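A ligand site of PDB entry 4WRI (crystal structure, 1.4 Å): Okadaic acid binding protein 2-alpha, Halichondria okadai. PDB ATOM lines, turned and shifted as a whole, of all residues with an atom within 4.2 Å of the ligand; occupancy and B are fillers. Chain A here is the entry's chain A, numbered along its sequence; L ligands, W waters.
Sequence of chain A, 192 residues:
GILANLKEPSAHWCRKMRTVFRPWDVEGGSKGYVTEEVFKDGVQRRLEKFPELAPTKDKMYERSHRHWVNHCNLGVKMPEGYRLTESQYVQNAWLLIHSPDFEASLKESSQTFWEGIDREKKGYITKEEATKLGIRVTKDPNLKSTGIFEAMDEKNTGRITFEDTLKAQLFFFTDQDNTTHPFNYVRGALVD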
ATOM      1  N   TRP A  24      -3.118  -0.080   2.511  1.00  0.00           N
ATOM      2  CA  TRP A  24      -3.212   1.116   3.322  1.00  0.00           C
ATOM      3  C   TRP A  24      -2.052   1.174   4.301  1.00  0.00           C
ATOM      4  O   TRP A  24      -1.451   2.223   4.525  1.00  0.00           O
ATOM      5  CB  TRP A  24      -4.514   1.149   4.104  1.00  0.00           C
ATOM      6  CG  TRP A  24      -5.760   1.031   3.266  1.00  0.00           C
ATOM      7  CD1 TRP A  24      -5.917   1.384   1.947  1.00  0.00           C
ATOM      8  CD2 TRP A  24      -7.036   0.587   3.715  1.00  0.00           C
ATOM      9  NE1 TRP A  24      -7.220   1.156   1.554  1.00  0.00           N
ATOM     10  CE2 TRP A  24      -7.916   0.639   2.622  1.00  0.00           C
ATOM     11  CE3 TRP A  24      -7.508   0.087   4.940  1.00  0.00           C
ATOM     12  CZ2 TRP A  24      -9.260   0.251   2.711  1.00  0.00           C
ATOM     13  CZ3 TRP A  24      -8.850  -0.285   5.024  1.00  0.00           C
ATOM     14  CH2 TRP A  24      -9.692  -0.222   3.917  1.00  0.00           C
ATOM     15  N   PHE A  39      -5.112   8.366   5.066  1.00  0.00           N
ATOM     16  CA  PHE A  39      -6.137   8.436   4.028  1.00  0.00           C
ATOM     17  C   PHE A  39      -6.237   9.810   3.400  1.00  0.00           C
ATOM     18  O   PHE A  39      -6.479   9.915   2.199  1.00  0.00           O
ATOM     19  CB  PHE A  39      -7.461   7.925   4.566  1.00  0.00           C
ATOM     20  CG  PHE A  39      -7.404   6.467   4.926  1.00  0.00           C
ATOM     21  CD1 PHE A  39      -7.250   5.510   3.938  1.00  0.00           C
ATOM     22  CD2 PHE A  39      -7.493   6.063   6.255  1.00  0.00           C
ATOM     23  CE1 PHE A  39      -7.162   4.160   4.265  1.00  0.00           C
ATOM     24  CE2 PHE A  39      -7.399   4.702   6.589  1.00  0.00           C
ATOM     25  CZ  PHE A  39      -7.250   3.758   5.584  1.00  0.00           C
ATOM     26  N   VAL A  43      -5.268  10.848  -0.926  1.00  0.00           N
ATOM     27  CA  VAL A  43      -6.096  11.474  -1.952  1.00  0.00           C
ATOM     28  C   VAL A  43      -5.272  11.841  -3.166  1.00  0.00           C
ATOM     29  O   VAL A  43      -5.625  11.490  -4.292  1.00  0.00           O
ATOM     30  CB  VAL A  43      -6.804  12.737  -1.415  1.00  0.00           C
ATOM     31  CG1 VAL A  43      -7.271  13.597  -2.578  1.00  0.00           C
ATOM     32  CG2 VAL A  43      -7.948  12.333  -0.523  1.00  0.00           C
ATOM     33  N   ARG A  46      -4.190   8.770  -5.135  1.00  0.00           N
ATOM     34  CA  ARG A  46      -5.286   8.236  -5.922  1.00  0.00           C
ATOM     35  C   ARG A  46      -5.571   9.052  -7.177  1.00  0.00           C
ATOM     36  O   ARG A  46      -5.924   8.497  -8.215  1.00  0.00           O
ATOM     37  CB  ARG A  46      -6.537   8.084  -5.049  1.00  0.00           C
ATOM     38  CG  ARG A  46      -6.391   6.887  -4.121  1.00  0.00           C
ATOM     39  CD  ARG A  46      -7.314   6.892  -2.927  1.00  0.00           C
ATOM     40  NE  ARG A  46      -7.143   5.616  -2.205  1.00  0.00           N
ATOM     41  CZ  ARG A  46      -6.107   5.342  -1.418  1.00  0.00           C
ATOM     42  NH1 ARG A  46      -5.160   6.234  -1.223  1.00  0.00           N
ATOM     43  NH2 ARG A  46      -6.013   4.142  -0.837  1.00  0.00           N
ATOM     44  N   PHE A  50      -5.345   7.284 -10.642  1.00  0.00           N
ATOM     45  CA  PHE A  50      -6.623   7.202 -11.301  1.00  0.00           C
ATOM     46  C   PHE A  50      -7.096   8.584 -11.687  1.00  0.00           C
ATOM     47  O   PHE A  50      -7.983   9.144 -11.072  1.00  0.00           O
ATOM     48  CB  PHE A  50      -7.641   6.505 -10.381  1.00  0.00           C
ATOM     49  CG  PHE A  50      -7.341   5.049 -10.230  1.00  0.00           C
ATOM     50  CD1 PHE A  50      -7.631   4.178 -11.275  1.00  0.00           C
ATOM     51  CD2 PHE A  50      -6.708   4.578  -9.106  1.00  0.00           C
ATOM     52  CE1 PHE A  50      -7.327   2.832 -11.160  1.00  0.00           C
ATOM     53  CE2 PHE A  50      -6.390   3.230  -8.989  1.00  0.00           C
ATOM     54  CZ  PHE A  50      -6.702   2.374 -10.011  1.00  0.00           C
ATOM     55  N   MET A  60     -13.025  14.274  -2.920  1.00  0.00           N
ATOM     56  CA  MET A  60     -12.138  13.225  -2.428  1.00  0.00           C
ATOM     57  C   MET A  60     -11.793  13.357  -0.953  1.00  0.00           C
ATOM     58  O   MET A  60     -11.709  12.361  -0.228  1.00  0.00           O
ATOM     59  CB  MET A  60     -10.857  13.167  -3.243  1.00  0.00           C
ATOM     60  CG  MET A  60     -11.107  12.748  -4.659  1.00  0.00           C
ATOM     61  SD  MET A  60     -11.255  10.964  -4.816  1.00  0.00           S
ATOM     62  CE  MET A  60      -9.518  10.494  -4.738  1.00  0.00           C
ATOM     63  N   ARG A  63     -14.533  11.895   0.917  1.00  0.00           N
ATOM     64  CA  ARG A  63     -14.522  10.440   0.763  1.00  0.00           C
ATOM     65  C   ARG A  63     -13.471   9.814   1.674  1.00  0.00           C
ATOM     66  O   ARG A  63     -13.737   8.771   2.284  1.00  0.00           O
ATOM     67  CB  ARG A  63     -14.277  10.048  -0.689  1.00  0.00           C
ATOM     68  CG  ARG A  63     -15.442  10.358  -1.604  1.00  0.00           C
ATOM     69  CD  ARG A  63     -15.018  10.273  -3.058  1.00  0.00           C
ATOM     70  NE  ARG A  63     -16.102  10.621  -3.984  1.00  0.00           N
ATOM     71  CZ  ARG A  63     -15.929  10.966  -5.261  1.00  0.00           C
ATOM     72  NH1 ARG A  63     -14.705  11.029  -5.773  1.00  0.00           N
ATOM     73  NH2 ARG A  63     -16.981  11.244  -6.016  1.00  0.00           N
ATOM     74  N   SER A  64     -12.290  10.409   1.767  1.00  0.00           N
ATOM     75  CA  SER A  64     -11.266   9.865   2.640  1.00  0.00           C
ATOM     76  C   SER A  64     -11.699   9.940   4.101  1.00  0.00           C
ATOM     77  O   SER A  64     -11.557   8.991   4.859  1.00  0.00           O
ATOM     78  CB  SER A  64      -9.906  10.536   2.428  1.00  0.00           C
ATOM     79  OG  SER A  64      -9.918  11.888   2.875  1.00  0.00           O
ATOM     80  N   HIS A  67     -14.403   7.480   4.819  1.00  0.00           N
ATOM     81  CA  HIS A  67     -13.829   6.144   4.849  1.00  0.00           C
ATOM     82  C   HIS A  67     -13.237   5.873   6.241  1.00  0.00           C
ATOM     83  O   HIS A  67     -13.453   4.802   6.814  1.00  0.00           O
ATOM     84  CB  HIS A  67     -12.757   5.981   3.785  1.00  0.00           C
ATOM     85  CG  HIS A  67     -12.028   4.680   3.864  1.00  0.00           C
ATOM     86  ND1 HIS A  67     -12.618   3.484   3.547  1.00  0.00           N
ATOM     87  CD2 HIS A  67     -10.764   4.396   4.267  1.00  0.00           C
ATOM     88  CE1 HIS A  67     -11.738   2.506   3.733  1.00  0.00           C
ATOM     89  NE2 HIS A  67     -10.607   3.038   4.161  1.00  0.00           N
ATOM     90  N   LEU A 106     -21.130  -0.372   0.187  1.00  0.00           N
ATOM     91  CA  LEU A 106     -20.190  -0.822  -0.831  1.00  0.00           C
ATOM     92  C   LEU A 106     -20.639  -0.314  -2.189  1.00  0.00           C
ATOM     93  O   LEU A 106     -19.813   0.129  -2.982  1.00  0.00           O
ATOM     94  CB  LEU A 106     -20.084  -2.347  -0.904  1.00  0.00           C
ATOM     95  CG  LEU A 106     -19.280  -3.072   0.149  1.00  0.00           C
ATOM     96  CD1 LEU A 106     -19.307  -4.547  -0.176  1.00  0.00           C
ATOM     97  CD2 LEU A 106     -17.852  -2.546   0.212  1.00  0.00           C
ATOM     98  N   SER A 109     -19.991   3.522  -2.575  1.00  0.00           N
ATOM     99  CA  SER A 109     -18.569   3.767  -2.802  1.00  0.00           C
ATOM    100  C   SER A 109     -18.160   3.336  -4.208  1.00  0.00           C
ATOM    101  O   SER A 109     -17.442   4.045  -4.909  1.00  0.00           O
ATOM    102  CB  SER A 109     -17.714   3.029  -1.780  1.00  0.00           C
ATOM    103  OG  SER A 109     -17.962   3.512  -0.478  1.00  0.00           O
ATOM    104  N   SER A 110     -18.626   2.171  -4.629  1.00  0.00           N
ATOM    105  CA  SER A 110     -18.237   1.654  -5.939  1.00  0.00           C
ATOM    106  C   SER A 110     -18.746   2.574  -7.054  1.00  0.00           C
ATOM    107  O   SER A 110     -18.077   2.762  -8.080  1.00  0.00           O
ATOM    108  CB  SER A 110     -18.742   0.237  -6.112  1.00  0.00           C
ATOM    109  OG  SER A 110     -17.980  -0.648  -5.300  1.00  0.00           O
ATOM    110  N   THR A 112     -18.883   5.763  -7.011  1.00  0.00           N
ATOM    111  CA  THR A 112     -17.946   6.870  -7.211  1.00  0.00           C
ATOM    112  C   THR A 112     -16.806   6.505  -8.158  1.00  0.00           C
ATOM    113  O   THR A 112     -16.390   7.337  -8.975  1.00  0.00           O
ATOM    114  CB  THR A 112     -17.393   7.444  -5.891  1.00  0.00           C
ATOM    115  OG1 THR A 112     -16.561   6.483  -5.236  1.00  0.00           O
ATOM    116  CG2 THR A 112     -18.543   7.827  -4.992  1.00  0.00           C
ATOM    117  N   PHE A 113     -16.339   5.274  -8.113  1.00  0.00           N
ATOM    118  CA  PHE A 113     -15.291   4.852  -9.015  1.00  0.00           C
ATOM    119  C   PHE A 113     -15.856   4.620 -10.408  1.00  0.00           C
ATOM    120  O   PHE A 113     -15.265   5.047 -11.401  1.00  0.00           O
ATOM    121  CB  PHE A 113     -14.630   3.560  -8.503  1.00  0.00           C
ATOM    122  CG  PHE A 113     -13.426   3.146  -9.301  1.00  0.00           C
ATOM    123  CD1 PHE A 113     -12.208   3.761  -9.101  1.00  0.00           C
ATOM    124  CD2 PHE A 113     -13.505   2.146 -10.263  1.00  0.00           C
ATOM    125  CE1 PHE A 113     -11.085   3.394  -9.827  1.00  0.00           C
ATOM    126  CE2 PHE A 113     -12.381   1.779 -10.989  1.00  0.00           C
ATOM    127  CZ  PHE A 113     -11.172   2.408 -10.764  1.00  0.00           C
ATOM    128  N   TRP A 114     -16.985   3.924 -10.457  1.00  0.00           N
ATOM    129  CA  TRP A 114     -17.594   3.522 -11.723  1.00  0.00           C
ATOM    130  C   TRP A 114     -17.951   4.728 -12.584  1.00  0.00           C
ATOM    131  O   TRP A 114     -17.832   4.676 -13.814  1.00  0.00           O
ATOM    132  CB  TRP A 114     -18.816   2.623 -11.480  1.00  0.00           C
ATOM    133  CG  TRP A 114     -19.304   2.041 -12.743  1.00  0.00           C
ATOM    134  CD1 TRP A 114     -20.214   2.589 -13.602  1.00  0.00           C
ATOM    135  CD2 TRP A 114     -18.864   0.821 -13.346  1.00  0.00           C
ATOM    136  NE1 TRP A 114     -20.384   1.773 -14.691  1.00  0.00           N
ATOM    137  CE2 TRP A 114     -19.541   0.694 -14.576  1.00  0.00           C
ATOM    138  CE3 TRP A 114     -17.950  -0.172 -12.971  1.00  0.00           C
ATOM    139  CZ2 TRP A 114     -19.366  -0.405 -15.419  1.00  0.00           C
ATOM    140  CZ3 TRP A 114     -17.773  -1.255 -13.819  1.00  0.00           C
ATOM    141  CH2 TRP A 114     -18.477  -1.356 -15.032  1.00  0.00           C
ATOM    142  N   ILE A 117     -15.011   5.951 -14.699  1.00  0.00           N
ATOM    143  CA  ILE A 117     -14.542   5.104 -15.786  1.00  0.00           C
ATOM    144  C   ILE A 117     -15.634   4.857 -16.813  1.00  0.00           C
ATOM    145  O   ILE A 117     -15.382   4.354 -17.909  1.00  0.00           O
ATOM    146  CB  ILE A 117     -14.014   3.755 -15.266  1.00  0.00           C
ATOM    147  CG1 ILE A 117     -15.166   2.994 -14.595  1.00  0.00           C
ATOM    148  CG2 ILE A 117     -12.815   4.000 -14.334  1.00  0.00           C
ATOM    149  CD1 ILE A 117     -14.828   1.679 -13.975  1.00  0.00           C
ATOM    150  N   ALA A 130     -11.865  -3.824 -18.535  1.00  0.00           N
ATOM    151  CA  ALA A 130     -11.984  -4.277 -17.130  1.00  0.00           C
ATOM    152  C   ALA A 130     -10.704  -4.930 -16.642  1.00  0.00           C
ATOM    153  O   ALA A 130     -10.334  -4.767 -15.473  1.00  0.00           O
ATOM    154  CB  ALA A 130     -13.155  -5.220 -16.961  1.00  0.00           C
ATOM    155  N   LEU A 133      -8.079  -2.129 -16.186  1.00  0.00           N
ATOM    156  CA  LEU A 133      -8.449  -1.323 -15.018  1.00  0.00           C
ATOM    157  C   LEU A 133      -8.266  -2.119 -13.723  1.00  0.00           C
ATOM    158  O   LEU A 133      -7.777  -1.594 -12.725  1.00  0.00           O
ATOM    159  CB  LEU A 133      -9.877  -0.870 -15.155  1.00  0.00           C
ATOM    160  CG  LEU A 133     -10.359   0.265 -14.267  1.00  0.00           C
ATOM    161  CD1 LEU A 133      -9.525   1.517 -14.480  1.00  0.00           C
ATOM    162  CD2 LEU A 133     -11.782   0.535 -14.648  1.00  0.00           C
ATOM    163  N   GLY A 134      -8.643  -3.398 -13.749  1.00  0.00           N
ATOM    164  CA  GLY A 134      -8.461  -4.247 -12.580  1.00  0.00           C
ATOM    165  C   GLY A 134      -7.017  -4.394 -12.164  1.00  0.00           C
ATOM    166  O   GLY A 134      -6.704  -4.414 -10.980  1.00  0.00           O
ATOM    167  N   VAL A 137      -6.223  -1.181 -10.422  1.00  0.00           N
ATOM    168  CA  VAL A 137      -6.863  -1.093  -9.117  1.00  0.00           C
ATOM    169  C   VAL A 137      -6.154  -1.961  -8.070  1.00  0.00           C
ATOM    170  O   VAL A 137      -5.909  -1.518  -6.934  1.00  0.00           O
ATOM    171  CB  VAL A 137      -8.339  -1.519  -9.203  1.00  0.00           C
ATOM    172  CG1 VAL A 137      -8.917  -1.864  -7.829  1.00  0.00           C
ATOM    173  CG2 VAL A 137      -9.165  -0.431  -9.898  1.00  0.00           C
ATOM    174  N   LEU A 143      -3.652 -10.539 -12.470  1.00  0.00           N
ATOM    175  CA  LEU A 143      -5.084 -10.597 -12.200  1.00  0.00           C
ATOM    176  C   LEU A 143      -5.873 -11.428 -13.208  1.00  0.00           C
ATOM    177  O   LEU A 143      -6.826 -12.096 -12.825  1.00  0.00           O
ATOM    178  CB  LEU A 143      -5.655  -9.178 -12.105  1.00  0.00           C
ATOM    179  CG  LEU A 143      -7.061  -9.124 -11.517  1.00  0.00           C
ATOM    180  CD1 LEU A 143      -7.085  -9.473 -10.056  1.00  0.00           C
ATOM    181  CD2 LEU A 143      -7.632  -7.714 -11.712  1.00  0.00           C
ATOM    182  N   ILE A 148     -11.104 -14.299 -12.667  1.00  0.00           N
ATOM    183  CA  ILE A 148     -12.213 -13.455 -12.231  1.00  0.00           C
ATOM    184  C   ILE A 148     -13.025 -12.860 -13.405  1.00  0.00           C
ATOM    185  O   ILE A 148     -14.239 -12.717 -13.288  1.00  0.00           O
ATOM    186  CB  ILE A 148     -11.747 -12.380 -11.235  1.00  0.00           C
ATOM    187  CG1 ILE A 148     -12.961 -11.792 -10.506  1.00  0.00           C
ATOM    188  CG2 ILE A 148     -10.885 -11.344 -11.925  1.00  0.00           C
ATOM    189  CD1 ILE A 148     -12.593 -10.897  -9.327  1.00  0.00           C
ATOM    190  N   PHE A 149     -12.393 -12.610 -14.540  1.00  0.00           N
ATOM    191  CA  PHE A 149     -13.133 -12.043 -15.663  1.00  0.00           C
ATOM    192  C   PHE A 149     -14.054 -13.058 -16.323  1.00  0.00           C
ATOM    193  O   PHE A 149     -15.146 -12.713 -16.772  1.00  0.00           O
ATOM    194  CB  PHE A 149     -12.176 -11.349 -16.632  1.00  0.00           C
ATOM    195  CG  PHE A 149     -11.447 -10.236 -15.969  1.00  0.00           C
ATOM    196  CD1 PHE A 149     -12.093  -9.029 -15.753  1.00  0.00           C
ATOM    197  CD2 PHE A 149     -10.176 -10.414 -15.465  1.00  0.00           C
ATOM    198  CE1 PHE A 149     -11.458  -8.009 -15.067  1.00  0.00           C
ATOM    199  CE2 PHE A 149      -9.526  -9.389 -14.797  1.00  0.00           C
ATOM    200  CZ  PHE A 149     -10.170  -8.178 -14.590  1.00  0.00           C
ATOM    201  N   MET A 152     -17.060 -13.491 -13.781  1.00  0.00           N
ATOM    202  CA  MET A 152     -17.996 -12.382 -13.863  1.00  0.00           C
ATOM    203  C   MET A 152     -18.833 -12.437 -15.148  1.00  0.00           C
ATOM    204  O   MET A 152     -20.052 -12.323 -15.095  1.00  0.00           O
ATOM    205  CB  MET A 152     -17.276 -11.031 -13.788  1.00  0.00           C
ATOM    206  CG  MET A 152     -16.790 -10.707 -12.391  1.00  0.00           C
ATOM    207  SD  MET A 152     -16.205  -8.992 -12.330  1.00  0.00           S
ATOM    208  CE  MET A 152     -14.771  -9.151 -13.388  1.00  0.00           C
ATOM    209  N   THR A 165     -19.309  -6.469 -11.046  1.00  0.00           N
ATOM    210  CA  THR A 165     -18.237  -6.117 -10.122  1.00  0.00           C
ATOM    211  C   THR A 165     -18.759  -6.018  -8.695  1.00  0.00           C
ATOM    212  O   THR A 165     -18.054  -6.388  -7.762  1.00  0.00           O
ATOM    213  CB  THR A 165     -17.477  -4.840 -10.547  1.00  0.00           C
ATOM    214  OG1 THR A 165     -18.284  -3.664 -10.305  1.00  0.00           O
ATOM    215  CG2 THR A 165     -17.085  -4.906 -12.030  1.00  0.00           C
ATOM    216  N   GLN A 169     -17.403  -8.265  -5.530  1.00  0.00           N
ATOM    217  CA  GLN A 169     -16.943  -7.560  -4.355  1.00  0.00           C
ATOM    218  C   GLN A 169     -17.722  -7.940  -3.088  1.00  0.00           C
ATOM    219  O   GLN A 169     -17.153  -8.049  -1.983  1.00  0.00           O
ATOM    220  CB  GLN A 169     -17.025  -6.077  -4.634  1.00  0.00           C
ATOM    221  CG  GLN A 169     -16.620  -5.204  -3.502  1.00  0.00           C
ATOM    222  CD  GLN A 169     -16.657  -3.774  -3.955  1.00  0.00           C
ATOM    223  OE1 GLN A 169     -15.615  -3.223  -4.316  1.00  0.00           O
ATOM    224  NE2 GLN A 169     -17.861  -3.187  -4.012  1.00  0.00           N
ATOM    225  N   PHE A 173     -16.200  -9.551   0.379  1.00  0.00           N
ATOM    226  CA  PHE A 173     -16.320  -8.940   1.707  1.00  0.00           C
ATOM    227  C   PHE A 173     -17.126  -9.776   2.695  1.00  0.00           C
ATOM    228  O   PHE A 173     -17.035  -9.532   3.885  1.00  0.00           O
ATOM    229  CB  PHE A 173     -16.877  -7.508   1.638  1.00  0.00           C
ATOM    230  CG  PHE A 173     -15.806  -6.465   1.472  1.00  0.00           C
ATOM    231  CD1 PHE A 173     -15.087  -6.000   2.569  1.00  0.00           C
ATOM    232  CD2 PHE A 173     -15.522  -5.951   0.212  1.00  0.00           C
ATOM    233  CE1 PHE A 173     -14.087  -5.038   2.410  1.00  0.00           C
ATOM    234  CE2 PHE A 173     -14.515  -4.996   0.051  1.00  0.00           C
ATOM    235  CZ  PHE A 173     -13.805  -4.554   1.150  1.00  0.00           C
ATOM    236  N   VAL A 186     -10.889 -10.351  -6.165  1.00  0.00           N
ATOM    237  CA  VAL A 186     -11.388  -9.064  -6.662  1.00  0.00           C
ATOM    238  C   VAL A 186     -10.468  -7.919  -6.244  1.00  0.00           C
ATOM    239  O   VAL A 186     -10.433  -6.895  -6.916  1.00  0.00           O
ATOM    240  CB  VAL A 186     -12.834  -8.820  -6.203  1.00  0.00           C
ATOM    241  CG1 VAL A 186     -12.867  -8.427  -4.740  1.00  0.00           C
ATOM    242  CG2 VAL A 186     -13.513  -7.757  -7.084  1.00  0.00           C
ATOM    243  N   ARG A 187      -9.687  -8.084  -5.179  1.00  0.00           N
ATOM    244  CA  ARG A 187      -8.692  -7.101  -4.778  1.00  0.00           C
ATOM    245  C   ARG A 187      -7.266  -7.548  -5.065  1.00  0.00           C
ATOM    246  O   ARG A 187      -6.289  -6.985  -4.556  1.00  0.00           O
ATOM    247  CB  ARG A 187      -8.863  -6.731  -3.294  1.00  0.00           C
ATOM    248  CG  ARG A 187     -10.272  -6.232  -2.988  1.00  0.00           C
ATOM    249  CD  ARG A 187     -10.396  -5.635  -1.623  1.00  0.00           C
ATOM    250  NE  ARG A 187      -9.797  -4.306  -1.471  1.00  0.00           N
ATOM    251  CZ  ARG A 187     -10.457  -3.180  -1.700  1.00  0.00           C
ATOM    252  NH1 ARG A 187     -11.696  -3.216  -2.179  1.00  0.00           N
ATOM    253  NH2 ARG A 187      -9.850  -2.022  -1.448  1.00  0.00           N
HETATM  254  C1  LIG L   1      -9.278   2.946  -3.841  1.00  0.00           C
HETATM  255  C2  LIG L   1      -9.652   3.906  -5.002  1.00  0.00           C
HETATM  256  C3  LIG L   1     -11.164   3.898  -5.224  1.00  0.00           C
HETATM  257  C4  LIG L   1     -11.969   4.305  -3.973  1.00  0.00           C
HETATM  258  C5  LIG L   1     -13.459   4.155  -4.262  1.00  0.00           C
HETATM  259  C6  LIG L   1     -14.296   4.758  -3.138  1.00  0.00           C
HETATM  260  C7  LIG L   1     -13.842   6.208  -2.842  1.00  0.00           C
HETATM  261  C8  LIG L   1     -12.349   6.198  -2.565  1.00  0.00           C
HETATM  262  C9  LIG L   1     -11.842   7.615  -2.436  1.00  0.00           C
HETATM  263  C10 LIG L   1     -11.012   7.944  -1.438  1.00  0.00           C
HETATM  264  C11 LIG L   1     -10.588   6.984  -0.368  1.00  0.00           C
HETATM  265  C12 LIG L   1     -10.878   5.541  -0.857  1.00  0.00           C
HETATM  266  C13 LIG L   1     -10.842   4.566   0.329  1.00  0.00           C
HETATM  267  C14 LIG L   1     -11.078   3.129  -0.206  1.00  0.00           C
HETATM  268  C15 LIG L   1     -12.186   2.473   0.165  1.00  0.00           C
HETATM  269  C16 LIG L   1     -12.393   1.101  -0.408  1.00  0.00           C
HETATM  270  C17 LIG L   1     -12.697  -0.026   0.615  1.00  0.00           C
HETATM  271  C18 LIG L   1     -13.782  -0.882  -0.070  1.00  0.00           C
HETATM  272  C19 LIG L   1     -14.078  -0.101  -1.392  1.00  0.00           C
HETATM  273  C20 LIG L   1     -15.482  -0.195  -1.812  1.00  0.00           C
HETATM  274  C21 LIG L   1     -15.651   0.570  -3.149  1.00  0.00           C
HETATM  275  C22 LIG L   1     -14.674  -0.047  -4.147  1.00  0.00           C
HETATM  276  C23 LIG L   1     -13.252   0.055  -3.583  1.00  0.00           C
HETATM  277  C24 LIG L   1     -12.252  -0.624  -4.579  1.00  0.00           C
HETATM  278  C25 LIG L   1     -12.484   0.065  -5.905  1.00  0.00           C
HETATM  279  C26 LIG L   1     -13.893   0.146  -6.372  1.00  0.00           C
HETATM  280  C27 LIG L   1     -14.402  -1.214  -6.897  1.00  0.00           C
HETATM  281  C28 LIG L   1     -13.632  -1.561  -8.184  1.00  0.00           C
HETATM  282  C29 LIG L   1     -14.150  -2.790  -8.930  1.00  0.00           C
HETATM  283  C30 LIG L   1     -13.154  -3.037 -10.106  1.00  0.00           C
HETATM  284  C31 LIG L   1     -13.129  -1.990 -11.186  1.00  0.00           C
HETATM  285  C32 LIG L   1     -12.259  -2.408 -12.370  1.00  0.00           C
HETATM  286  C33 LIG L   1     -12.468  -3.857 -12.810  1.00  0.00           C
HETATM  287  C34 LIG L   1     -12.587  -4.767 -11.576  1.00  0.00           C
HETATM  288  C35 LIG L   1     -13.128  -6.151 -12.070  1.00  0.00           C
HETATM  289  C36 LIG L   1     -12.983  -7.141 -10.921  1.00  0.00           C
HETATM  290  C37 LIG L   1     -11.545  -7.147 -10.479  1.00  0.00           C
HETATM  291  C38 LIG L   1     -11.050  -5.787 -10.061  1.00  0.00           C
HETATM  292  C39 LIG L   1     -14.529  -1.615 -11.677  1.00  0.00           C
HETATM  293  C40 LIG L   1     -14.105  -4.013  -8.000  1.00  0.00           C
HETATM  294  C41 LIG L   1     -11.537   0.576  -6.630  1.00  0.00           C
HETATM  295  C42 LIG L   1      -9.476   4.565   0.978  1.00  0.00           C
HETATM  296  C43 LIG L   1     -10.544   9.380  -1.423  1.00  0.00           C
HETATM  297  C44 LIG L   1      -8.925   3.485  -6.266  1.00  0.00           C
HETATM  298  O1  LIG L   1      -9.709   1.795  -3.967  1.00  0.00           O
HETATM  299  O2  LIG L   1      -8.622   3.375  -2.891  1.00  0.00           O
HETATM  300  O3  LIG L   1      -9.238   5.226  -4.671  1.00  0.00           O
HETATM  301  O4  LIG L   1     -11.649   5.672  -3.677  1.00  0.00           O
HETATM  302  O5  LIG L   1     -14.602   6.716  -1.711  1.00  0.00           O
HETATM  303  O6  LIG L   1     -12.126   5.440  -1.381  1.00  0.00           O
HETATM  304  O7  LIG L   1     -13.583   1.186  -1.128  1.00  0.00           O
HETATM  305  O8  LIG L   1     -13.179  -0.683  -2.375  1.00  0.00           O
HETATM  306  O9  LIG L   1     -14.791   0.670  -5.377  1.00  0.00           O
HETATM  307  O10 LIG L   1     -10.965  -0.516  -4.101  1.00  0.00           O
HETATM  308  O11 LIG L   1     -15.782  -1.061  -7.208  1.00  0.00           O
HETATM  309  O12 LIG L   1     -13.520  -4.337 -10.670  1.00  0.00           O
HETATM  310  O13 LIG L   1     -11.251  -4.836 -11.155  1.00  0.00           O
HETATM  311  O   HOH W   1      -9.336  -2.882  -4.631  1.00  0.00           O
HETATM  312  O   HOH W   2     -15.589   4.981   0.233  1.00  0.00           O
HETATM  313  O   HOH W   3      -7.619   1.650  -1.219  1.00  0.00           O
HETATM  314  O   HOH W   4     -17.572  -3.225  -7.644  1.00  0.00           O
HETATM  315  O   HOH W   5     -13.870   7.170  -6.201  1.00  0.00           O
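The guanidinium group of Arg 46 is in salt-bridge range of an oxygen (O2) of the ligand.
The side-chain hydroxyl (OG) of Ser 110 sits at hydrogen-bond distance from an oxygen (O11) of the ligand, 2.9 Å away.
The guanidinium group of Arg 187 is in hydrogen-bond range of an oxygen (O8) of the ligand (2.9 Å).
Residues that only touch the ligand: Gly 134 (3.2 Å), Gln 169 (3.3 Å), Val 186 (3.4 Å), Met 60 (3.4 Å), Ser 109 (3.5 Å), Arg 63 (3.5 Å), Ala 130 (3.5 Å), His 67 (3.5 Å), Thr 112 (3.5 Å), Met 152 (3.7 Å), Phe 50 (3.7 Å), Leu 133 (3.8 Å), Val 137 (3.8 Å), Ser 64 (3.8 Å), Phe 39 (3.8 Å), Phe 113 (3.8 Å), Thr 165 (3.9 Å), Phe 173 (3.9 Å), Phe 149 (3.9 Å), Leu 106 (3.9 Å) and Trp 114 (3.9 Å).
Within 4 Å of the ligand: Phe 39, Arg 46, Phe 50, Met 60, Arg 63, Ser 64, His 67, Leu 106, Ser 109, Ser 110, Thr 112, Phe 113, Trp 114, Ala 130, Leu 133, Gly 134, Val 137, Phe 149, Met 152, Thr 165, Gln 169, Phe 173, Val 186 and Arg 187.
The nearest printed residue that does not touch the ligand is Ile 117 (4.03 Å).
Water W3 lies within hydrogen-bond range of an oxygen (O2) of the ligand (2.6 Å), the indole nitrogen of Trp 24 (2.8 Å) and the guanidinium group of Arg 46 (3.0 Å).
Water W2 lies within hydrogen-bond range of an oxygen (O5) of the ligand and the side-chain hydroxyl (OG) of Ser 109.
Water W4 bridges OG1 of Thr 165 and O11 of the ligand.
Water W1 lies within hydrogen-bond range of O10 of the ligand (2.9 Å) and NH2 of Arg 187 (3.3 Å).
The backbone carbonyl oxygen (O) of Ser 109 is in hydrogen-bond range of the side-chain hydroxyl (OG1) of Thr 112 (2.6 Å).
OG of Ser 110 is in hydrogen-bond range of O of Leu 106 (3.1 Å).
SD of Met 60 is in hydrogen-bond range of NH1 of Arg 63 (3.6 Å).
OG of Ser 110 is in hydrogen-bond range of NE2 of Gln 169 (2.8 Å).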
